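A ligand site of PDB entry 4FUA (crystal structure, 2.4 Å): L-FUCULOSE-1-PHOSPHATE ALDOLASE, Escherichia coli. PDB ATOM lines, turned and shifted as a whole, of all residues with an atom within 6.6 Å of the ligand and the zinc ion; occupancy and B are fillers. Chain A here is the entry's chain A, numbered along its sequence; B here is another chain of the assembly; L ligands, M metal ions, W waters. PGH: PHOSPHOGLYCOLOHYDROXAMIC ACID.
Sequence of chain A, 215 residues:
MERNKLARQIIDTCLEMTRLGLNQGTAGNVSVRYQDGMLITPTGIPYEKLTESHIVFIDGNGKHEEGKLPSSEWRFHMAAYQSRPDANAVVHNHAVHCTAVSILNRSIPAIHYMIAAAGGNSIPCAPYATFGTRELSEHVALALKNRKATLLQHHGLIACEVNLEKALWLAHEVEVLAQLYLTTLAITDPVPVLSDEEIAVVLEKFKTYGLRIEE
The side-chain hydroxyl of Tyr 113 of chain B sits close to an oxygen (O2) of the ligand (3.4 Å). ND2 of Asn 29 sits at hydrogen-bond distance from O4P of the ligand, at 2.9 Å. An oxygen (O3P) of the ligand is in hydrogen-bond range of the backbone NH (N) of Gly 44 (2.9 Å). An oxygen (O4P) of the ligand is in hydrogen-bond range of the side-chain hydroxyl (OG) of Ser 71 (2.6 Å). O2P of the ligand lies within hydrogen-bond range of N of Ser 72, 3.0 Å away. The side-chain hydroxyl (OG1) of Thr 43 lies within hydrogen-bond range of an oxygen (O2P) of the ligand (2.9 Å). The side-chain hydroxyl (OG) of Ser 72 lies within hydrogen-bond range of an oxygen (O2P) of the ligand (2.9 Å). An oxygen (O1) of the ligand sits close to the backbone NH (N) of Gly 28 (2.8 Å). The side-chain carboxylate (OE2) of Glu 73 is in hydrogen-bond range of a nitrogen (N2) of the ligand (3.1 Å).
The backbone carbonyl oxygen of Ala 27 is in hydrogen-bond range of the side-chain amide nitrogen of Asn 23, at 3.0 Å. The backbone NH of His 92 lies within hydrogen-bond range of the backbone carbonyl oxygen of Asn 29 (2.9 Å). The side-chain hydroxyl (OG) of Ser 71 sits at hydrogen-bond distance from the side-chain amide nitrogen (ND2) of Asn 29. OD1 of Asn 23 lies within hydrogen-bond range of N of His 94. The side-chain carboxylate (OE1) of Glu 73 sits at hydrogen-bond distance from the backbone NH (N) of Gly 132, at 2.9 Å. The backbone NH (N) of Glu 73 sits close to the side-chain hydroxyl (OG) of Ser 71, 3.2 Å away. The backbone NH (N) of Ser 71 sits at hydrogen-bond distance from the backbone carbonyl oxygen (O) of Thr 41, at 3.1 Å.
Thr 26 touches the ligand (O to O3P, 3.6 Å). C of Ala 27 touches O1 of the ligand, at 3.8 Å. The nearest printed residue that does not touch the ligand is Pro 42 (4.4 Å).
Residues that only touch the zinc ion: Tyr 113 of chain B and Glu 73. Within 4 Å of the zinc ion: Glu 73, His 92, His 94, His 155 and Tyr 113 of chain B. Along chain A the residues within 4 Å of the zinc ion span positions 73 to 155. The nearest printed residue that does not touch the zinc ion is Gly 28 (4.6 Å).
The zinc ion is bound by O2 of the ligand (1.9 Å), NE2 of His 155 (2.0 Å), NE2 of His 94 (2.0 Å), NE2 of His 92 (2.1 Å) and O1 of the ligand (2.2 Å).
Water W2 lies within hydrogen-bond range of O4P of the ligand (2.7 Å), OG1 of Thr 41 (2.7 Å), O of Pro 42 (3.1 Å) and O of Gly 28 (3.4 Å). Water W1 lies within hydrogen-bond range of OH of Tyr 113 of chain B and N2 of the ligand.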
ATOM      1  N   ASN A  23     -27.327  19.149   3.794  1.00  0.00           N
ATOM      2  CA  ASN A  23     -26.696  18.390   2.729  1.00  0.00           C
ATOM      3  C   ASN A  23     -25.735  17.393   3.335  1.00  0.00           C
ATOM      4  O   ASN A  23     -25.161  17.642   4.393  1.00  0.00           O
ATOM      5  CB  ASN A  23     -25.919  19.360   1.841  1.00  0.00           C
ATOM      6  CG  ASN A  23     -25.338  18.691   0.597  1.00  0.00           C
ATOM      7  OD1 ASN A  23     -26.072  18.240  -0.282  1.00  0.00           O
ATOM      8  ND2 ASN A  23     -24.003  18.662   0.509  1.00  0.00           N
ATOM      9  N   THR A  26     -22.035  13.073  -1.301  1.00  0.00           N
ATOM     10  CA  THR A  26     -21.319  13.696  -2.409  1.00  0.00           C
ATOM     11  C   THR A  26     -22.257  14.631  -3.161  1.00  0.00           C
ATOM     12  O   THR A  26     -21.904  15.187  -4.209  1.00  0.00           O
ATOM     13  CB  THR A  26     -20.731  12.622  -3.392  1.00  0.00           C
ATOM     14  OG1 THR A  26     -21.765  11.710  -3.804  1.00  0.00           O
ATOM     15  CG2 THR A  26     -19.612  11.843  -2.716  1.00  0.00           C
ATOM     16  N   ALA A  27     -23.454  14.816  -2.609  1.00  0.00           N
ATOM     17  CA  ALA A  27     -24.463  15.679  -3.193  1.00  0.00           C
ATOM     18  C   ALA A  27     -24.142  17.156  -3.014  1.00  0.00           C
ATOM     19  O   ALA A  27     -23.352  17.535  -2.146  1.00  0.00           O
ATOM     20  CB  ALA A  27     -25.818  15.354  -2.582  1.00  0.00           C
ATOM     21  N   GLY A  28     -24.746  17.987  -3.835  1.00  0.00           N
ATOM     22  CA  GLY A  28     -24.518  19.413  -3.723  1.00  0.00           C
ATOM     23  C   GLY A  28     -23.331  19.995  -4.459  1.00  0.00           C
ATOM     24  O   GLY A  28     -22.380  19.308  -4.826  1.00  0.00           O
ATOM     25  N   ASN A  29     -23.433  21.288  -4.714  1.00  0.00           N
ATOM     26  CA  ASN A  29     -22.412  22.054  -5.393  1.00  0.00           C
ATOM     27  C   ASN A  29     -22.622  23.534  -5.095  1.00  0.00           C
ATOM     28  O   ASN A  29     -23.713  23.976  -4.766  1.00  0.00           O
ATOM     29  CB  ASN A  29     -22.368  21.745  -6.906  1.00  0.00           C
ATOM     30  CG  ASN A  29     -23.719  21.361  -7.500  1.00  0.00           C
ATOM     31  OD1 ASN A  29     -24.549  22.213  -7.771  1.00  0.00           O
ATOM     32  ND2 ASN A  29     -23.925  20.064  -7.741  1.00  0.00           N
ATOM     33  N   VAL A  30     -21.537  24.284  -5.122  1.00  0.00           N
ATOM     34  CA  VAL A  30     -21.620  25.699  -4.827  1.00  0.00           C
ATOM     35  C   VAL A  30     -20.674  26.411  -5.754  1.00  0.00           C
ATOM     36  O   VAL A  30     -19.619  25.863  -6.089  1.00  0.00           O
ATOM     37  CB  VAL A  30     -21.166  25.990  -3.386  1.00  0.00           C
ATOM     38  CG1 VAL A  30     -21.142  27.454  -3.126  1.00  0.00           C
ATOM     39  CG2 VAL A  30     -22.082  25.296  -2.402  1.00  0.00           C
ATOM     40  N   ILE A  40     -16.521  27.200  -9.171  1.00  0.00           N
ATOM     41  CA  ILE A  40     -17.454  26.179  -8.742  1.00  0.00           C
ATOM     42  C   ILE A  40     -16.746  24.951  -8.206  1.00  0.00           C
ATOM     43  O   ILE A  40     -15.653  24.600  -8.645  1.00  0.00           O
ATOM     44  CB  ILE A  40     -18.376  25.750  -9.919  1.00  0.00           C
ATOM     45  CG1 ILE A  40     -19.554  24.907  -9.390  1.00  0.00           C
ATOM     46  CG2 ILE A  40     -17.583  24.986 -10.975  1.00  0.00           C
ATOM     47  CD1 ILE A  40     -20.670  24.723 -10.381  1.00  0.00           C
ATOM     48  N   THR A  41     -17.385  24.283  -7.255  1.00  0.00           N
ATOM     49  CA  THR A  41     -16.829  23.093  -6.653  1.00  0.00           C
ATOM     50  C   THR A  41     -16.665  22.026  -7.708  1.00  0.00           C
ATOM     51  O   THR A  41     -17.278  22.092  -8.768  1.00  0.00           O
ATOM     52  CB  THR A  41     -17.751  22.578  -5.535  1.00  0.00           C
ATOM     53  OG1 THR A  41     -19.095  22.534  -6.001  1.00  0.00           O
ATOM     54  CG2 THR A  41     -17.695  23.498  -4.342  1.00  0.00           C
ATOM     55  N   PRO A  42     -15.723  21.108  -7.490  1.00  0.00           N
ATOM     56  CA  PRO A  42     -15.511  20.041  -8.463  1.00  0.00           C
ATOM     57  C   PRO A  42     -16.430  18.862  -8.207  1.00  0.00           C
ATOM     58  O   PRO A  42     -16.854  18.609  -7.061  1.00  0.00           O
ATOM     59  CB  PRO A  42     -14.048  19.690  -8.232  1.00  0.00           C
ATOM     60  CG  PRO A  42     -13.902  19.853  -6.778  1.00  0.00           C
ATOM     61  CD  PRO A  42     -14.604  21.171  -6.542  1.00  0.00           C
ATOM     62  N   THR A  43     -16.686  18.140  -9.290  1.00  0.00           N
ATOM     63  CA  THR A  43     -17.561  16.979  -9.272  1.00  0.00           C
ATOM     64  C   THR A  43     -17.046  15.796  -8.464  1.00  0.00           C
ATOM     65  O   THR A  43     -15.929  15.307  -8.673  1.00  0.00           O
ATOM     66  CB  THR A  43     -17.913  16.502 -10.707  1.00  0.00           C
ATOM     67  OG1 THR A  43     -18.755  15.346 -10.633  1.00  0.00           O
ATOM     68  CG2 THR A  43     -16.662  16.140 -11.505  1.00  0.00           C
ATOM     69  N   GLY A  44     -17.864  15.377  -7.500  1.00  0.00           N
ATOM     70  CA  GLY A  44     -17.552  14.237  -6.670  1.00  0.00           C
ATOM     71  C   GLY A  44     -16.382  14.210  -5.707  1.00  0.00           C
ATOM     72  O   GLY A  44     -15.816  13.145  -5.485  1.00  0.00           O
ATOM     73  N   ILE A  45     -15.992  15.357  -5.154  1.00  0.00           N
ATOM     74  CA  ILE A  45     -14.889  15.348  -4.201  1.00  0.00           C
ATOM     75  C   ILE A  45     -15.424  15.801  -2.861  1.00  0.00           C
ATOM     76  O   ILE A  45     -15.905  16.921  -2.735  1.00  0.00           O
ATOM     77  CB  ILE A  45     -13.740  16.263  -4.636  1.00  0.00           C
ATOM     78  CG1 ILE A  45     -13.012  15.649  -5.842  1.00  0.00           C
ATOM     79  CG2 ILE A  45     -12.756  16.470  -3.501  1.00  0.00           C
ATOM     80  CD1 ILE A  45     -11.942  16.532  -6.434  1.00  0.00           C
ATOM     81  N   PRO A  70     -15.250  20.252 -13.396  1.00  0.00           N
ATOM     82  CA  PRO A  70     -16.239  21.051 -12.654  1.00  0.00           C
ATOM     83  C   PRO A  70     -17.470  20.215 -12.297  1.00  0.00           C
ATOM     84  O   PRO A  70     -17.645  19.105 -12.802  1.00  0.00           O
ATOM     85  CB  PRO A  70     -16.553  22.181 -13.629  1.00  0.00           C
ATOM     86  CG  PRO A  70     -16.417  21.541 -14.932  1.00  0.00           C
ATOM     87  CD  PRO A  70     -15.167  20.706 -14.788  1.00  0.00           C
ATOM     88  N   SER A  71     -18.277  20.744 -11.398  1.00  0.00           N
ATOM     89  CA  SER A  71     -19.495  20.061 -10.973  1.00  0.00           C
ATOM     90  C   SER A  71     -20.360  19.747 -12.181  1.00  0.00           C
ATOM     91  O   SER A  71     -20.519  20.582 -13.063  1.00  0.00           O
ATOM     92  CB  SER A  71     -20.287  20.943 -10.009  1.00  0.00           C
ATOM     93  OG  SER A  71     -21.613  20.497  -9.866  1.00  0.00           O
ATOM     94  N   SER A  72     -20.930  18.546 -12.198  1.00  0.00           N
ATOM     95  CA  SER A  72     -21.803  18.093 -13.276  1.00  0.00           C
ATOM     96  C   SER A  72     -22.950  19.078 -13.520  1.00  0.00           C
ATOM     97  O   SER A  72     -23.487  19.192 -14.617  1.00  0.00           O
ATOM     98  CB  SER A  72     -22.365  16.697 -12.973  1.00  0.00           C
ATOM     99  OG  SER A  72     -23.242  16.697 -11.843  1.00  0.00           O
ATOM    100  N   GLU A  73     -23.277  19.840 -12.484  1.00  0.00           N
ATOM    101  CA  GLU A  73     -24.360  20.794 -12.573  1.00  0.00           C
ATOM    102  C   GLU A  73     -23.916  22.173 -12.996  1.00  0.00           C
ATOM    103  O   GLU A  73     -24.738  23.088 -13.021  1.00  0.00           O
ATOM    104  CB  GLU A  73     -25.091  20.878 -11.235  1.00  0.00           C
ATOM    105  CG  GLU A  73     -25.551  19.536 -10.699  1.00  0.00           C
ATOM    106  CD  GLU A  73     -26.670  18.900 -11.522  1.00  0.00           C
ATOM    107  OE1 GLU A  73     -27.042  19.402 -12.607  1.00  0.00           O
ATOM    108  OE2 GLU A  73     -27.182  17.853 -11.063  1.00  0.00           O
ATOM    109  N   PHE A  76     -26.441  24.588 -14.807  1.00  0.00           N
ATOM    110  CA  PHE A  76     -27.545  25.264 -14.143  1.00  0.00           C
ATOM    111  C   PHE A  76     -27.111  26.351 -13.162  1.00  0.00           C
ATOM    112  O   PHE A  76     -27.950  27.062 -12.600  1.00  0.00           O
ATOM    113  CB  PHE A  76     -28.615  24.274 -13.593  1.00  0.00           C
ATOM    114  CG  PHE A  76     -28.287  23.621 -12.263  1.00  0.00           C
ATOM    115  CD1 PHE A  76     -27.621  24.277 -11.249  1.00  0.00           C
ATOM    116  CD2 PHE A  76     -28.776  22.331 -12.003  1.00  0.00           C
ATOM    117  CE1 PHE A  76     -27.446  23.689  -9.998  1.00  0.00           C
ATOM    118  CE2 PHE A  76     -28.607  21.726 -10.756  1.00  0.00           C
ATOM    119  CZ  PHE A  76     -27.944  22.404  -9.747  1.00  0.00           C
ATOM    120  N   HIS A  92     -26.495  24.652  -4.069  1.00  0.00           N
ATOM    121  CA  HIS A  92     -27.328  23.528  -4.428  1.00  0.00           C
ATOM    122  C   HIS A  92     -27.095  22.390  -3.464  1.00  0.00           C
ATOM    123  O   HIS A  92     -25.968  22.012  -3.218  1.00  0.00           O
ATOM    124  CB  HIS A  92     -27.017  23.015  -5.830  1.00  0.00           C
ATOM    125  CG  HIS A  92     -27.688  21.713  -6.142  1.00  0.00           C
ATOM    126  ND1 HIS A  92     -29.058  21.520  -6.096  1.00  0.00           N
ATOM    127  CD2 HIS A  92     -27.151  20.507  -6.460  1.00  0.00           C
ATOM    128  CE1 HIS A  92     -29.297  20.231  -6.375  1.00  0.00           C
ATOM    129  NE2 HIS A  92     -28.174  19.583  -6.609  1.00  0.00           N
ATOM    130  N   ASN A  93     -28.169  21.797  -2.988  1.00  0.00           N
ATOM    131  CA  ASN A  93     -28.041  20.677  -2.082  1.00  0.00           C
ATOM    132  C   ASN A  93     -29.215  19.743  -2.196  1.00  0.00           C
ATOM    133  O   ASN A  93     -30.216  20.078  -2.809  1.00  0.00           O
ATOM    134  CB  ASN A  93     -27.908  21.171  -0.657  1.00  0.00           C
ATOM    135  CG  ASN A  93     -29.089  21.961  -0.205  1.00  0.00           C
ATOM    136  OD1 ASN A  93     -30.244  21.557  -0.401  1.00  0.00           O
ATOM    137  ND2 ASN A  93     -28.827  23.094   0.413  1.00  0.00           N
ATOM    138  N   HIS A  94     -29.085  18.561  -1.599  1.00  0.00           N
ATOM    139  CA  HIS A  94     -30.192  17.592  -1.594  1.00  0.00           C
ATOM    140  C   HIS A  94     -30.768  17.507  -0.164  1.00  0.00           C
ATOM    141  O   HIS A  94     -30.899  16.428   0.418  1.00  0.00           O
ATOM    142  CB  HIS A  94     -29.725  16.216  -2.052  1.00  0.00           C
ATOM    143  CG  HIS A  94     -29.302  16.152  -3.492  1.00  0.00           C
ATOM    144  ND1 HIS A  94     -29.048  14.983  -4.158  1.00  0.00           N
ATOM    145  CD2 HIS A  94     -29.062  17.143  -4.386  1.00  0.00           C
ATOM    146  CE1 HIS A  94     -28.654  15.287  -5.416  1.00  0.00           C
ATOM    147  NE2 HIS A  94     -28.651  16.584  -5.602  1.00  0.00           N
ATOM    148  N   PHE A 131     -29.982  14.905 -14.324  1.00  0.00           N
ATOM    149  CA  PHE A 131     -29.010  15.786 -13.674  1.00  0.00           C
ATOM    150  C   PHE A 131     -27.892  16.080 -14.652  1.00  0.00           C
ATOM    151  O   PHE A 131     -27.631  15.286 -15.534  1.00  0.00           O
ATOM    152  CB  PHE A 131     -28.412  15.144 -12.411  1.00  0.00           C
ATOM    153  CG  PHE A 131     -27.485  14.020 -12.689  1.00  0.00           C
ATOM    154  CD1 PHE A 131     -26.140  14.269 -12.958  1.00  0.00           C
ATOM    155  CD2 PHE A 131     -27.952  12.711 -12.733  1.00  0.00           C
ATOM    156  CE1 PHE A 131     -25.285  13.216 -13.275  1.00  0.00           C
ATOM    157  CE2 PHE A 131     -27.105  11.656 -13.053  1.00  0.00           C
ATOM    158  CZ  PHE A 131     -25.761  11.904 -13.321  1.00  0.00           C
ATOM    159  N   GLY A 132     -27.286  17.259 -14.501  1.00  0.00           N
ATOM    160  CA  GLY A 132     -26.177  17.673 -15.356  1.00  0.00           C
ATOM    161  C   GLY A 132     -26.512  17.767 -16.837  1.00  0.00           C
ATOM    162  O   GLY A 132     -25.634  17.692 -17.689  1.00  0.00           O
ATOM    163  N   LEU A 136     -32.169  20.563 -18.039  1.00  0.00           N
ATOM    164  CA  LEU A 136     -32.367  20.805 -16.628  1.00  0.00           C
ATOM    165  C   LEU A 136     -32.088  22.279 -16.388  1.00  0.00           C
ATOM    166  O   LEU A 136     -32.683  22.902 -15.515  1.00  0.00           O
ATOM    167  CB  LEU A 136     -31.396  19.978 -15.803  1.00  0.00           C
ATOM    168  CG  LEU A 136     -31.780  19.493 -14.401  1.00  0.00           C
ATOM    169  CD1 LEU A 136     -30.527  19.482 -13.597  1.00  0.00           C
ATOM    170  CD2 LEU A 136     -32.824  20.357 -13.739  1.00  0.00           C
ATOM    171  N   LEU A 152     -36.131  21.253  -7.223  1.00  0.00           N
ATOM    172  CA  LEU A 152     -35.892  20.528  -8.474  1.00  0.00           C
ATOM    173  C   LEU A 152     -36.663  19.214  -8.294  1.00  0.00           C
ATOM    174  O   LEU A 152     -36.382  18.461  -7.354  1.00  0.00           O
ATOM    175  CB  LEU A 152     -34.385  20.275  -8.639  1.00  0.00           C
ATOM    176  CG  LEU A 152     -33.493  21.513  -8.542  1.00  0.00           C
ATOM    177  CD1 LEU A 152     -32.092  21.162  -8.097  1.00  0.00           C
ATOM    178  CD2 LEU A 152     -33.450  22.221  -9.849  1.00  0.00           C
ATOM    179  N   HIS A 155     -35.226  15.796  -7.143  1.00  0.00           N
ATOM    180  CA  HIS A 155     -33.797  16.082  -7.051  1.00  0.00           C
ATOM    181  C   HIS A 155     -33.337  16.790  -5.790  1.00  0.00           C
ATOM    182  O   HIS A 155     -32.618  16.208  -4.990  1.00  0.00           O
ATOM    183  CB  HIS A 155     -33.342  16.840  -8.295  1.00  0.00           C
ATOM    184  CG  HIS A 155     -31.859  17.012  -8.401  1.00  0.00           C
ATOM    185  ND1 HIS A 155     -31.172  17.035  -9.599  1.00  0.00           N
ATOM    186  CD2 HIS A 155     -30.928  17.188  -7.437  1.00  0.00           C
ATOM    187  CE1 HIS A 155     -29.881  17.228  -9.317  1.00  0.00           C
ATOM    188  NE2 HIS A 155     -29.677  17.332  -8.020  1.00  0.00           N
ATOM    189  N   GLY A 156     -33.656  18.075  -5.663  1.00  0.00           N
ATOM    190  CA  GLY A 156     -33.217  18.806  -4.486  1.00  0.00           C
ATOM    191  C   GLY A 156     -33.642  20.262  -4.466  1.00  0.00           C
ATOM    192  O   GLY A 156     -34.758  20.602  -4.843  1.00  0.00           O
ATOM    193  N   TYR B 113     -33.330  10.026  -8.220  1.00  0.00           N
ATOM    194  CA  TYR B 113     -32.369   9.473  -9.167  1.00  0.00           C
ATOM    195  C   TYR B 113     -31.158   8.797  -8.521  1.00  0.00           C
ATOM    196  O   TYR B 113     -30.451   8.025  -9.162  1.00  0.00           O
ATOM    197  CB  TYR B 113     -31.938  10.543 -10.170  1.00  0.00           C
ATOM    198  CG  TYR B 113     -30.898  11.516  -9.664  1.00  0.00           C
ATOM    199  CD1 TYR B 113     -29.542  11.164  -9.629  1.00  0.00           C
ATOM    200  CD2 TYR B 113     -31.253  12.779  -9.222  1.00  0.00           C
ATOM    201  CE1 TYR B 113     -28.591  12.054  -9.148  1.00  0.00           C
ATOM    202  CE2 TYR B 113     -30.302  13.668  -8.741  1.00  0.00           C
ATOM    203  CZ  TYR B 113     -28.973  13.293  -8.704  1.00  0.00           C
ATOM    204  OH  TYR B 113     -28.015  14.174  -8.267  1.00  0.00           O
HETATM  205  C1  PGH L   1     -25.122  17.009  -7.263  1.00  0.00           C
HETATM  206  C2  PGH L   1     -23.650  16.637  -7.010  1.00  0.00           C
HETATM  207  N2  PGH L   1     -25.535  16.947  -8.555  1.00  0.00           N
HETATM  208  O2  PGH L   1     -26.834  17.304  -8.729  1.00  0.00           O
HETATM  209  O1  PGH L   1     -25.886  17.336  -6.364  1.00  0.00           O
HETATM  210  O1P PGH L   1     -22.933  16.619  -8.229  1.00  0.00           O
HETATM  211  O2P PGH L   1     -21.148  16.776  -9.810  1.00  0.00           O
HETATM  212  O3P PGH L   1     -20.617  16.270  -7.340  1.00  0.00           O
HETATM  213  O4P PGH L   1     -21.435  18.613  -8.068  1.00  0.00           O
HETATM  214  P   PGH L   1     -21.464  17.053  -8.338  1.00  0.00           P
HETATM  215 ZN    ZN M   1     -27.877  17.553  -7.179  1.00  0.00          ZN
HETATM  216  O   HOH W   1     -24.983  13.702  -8.930  1.00  0.00           O
HETATM  217  O   HOH W   2     -19.632  20.011  -6.716  1.00  0.00           O
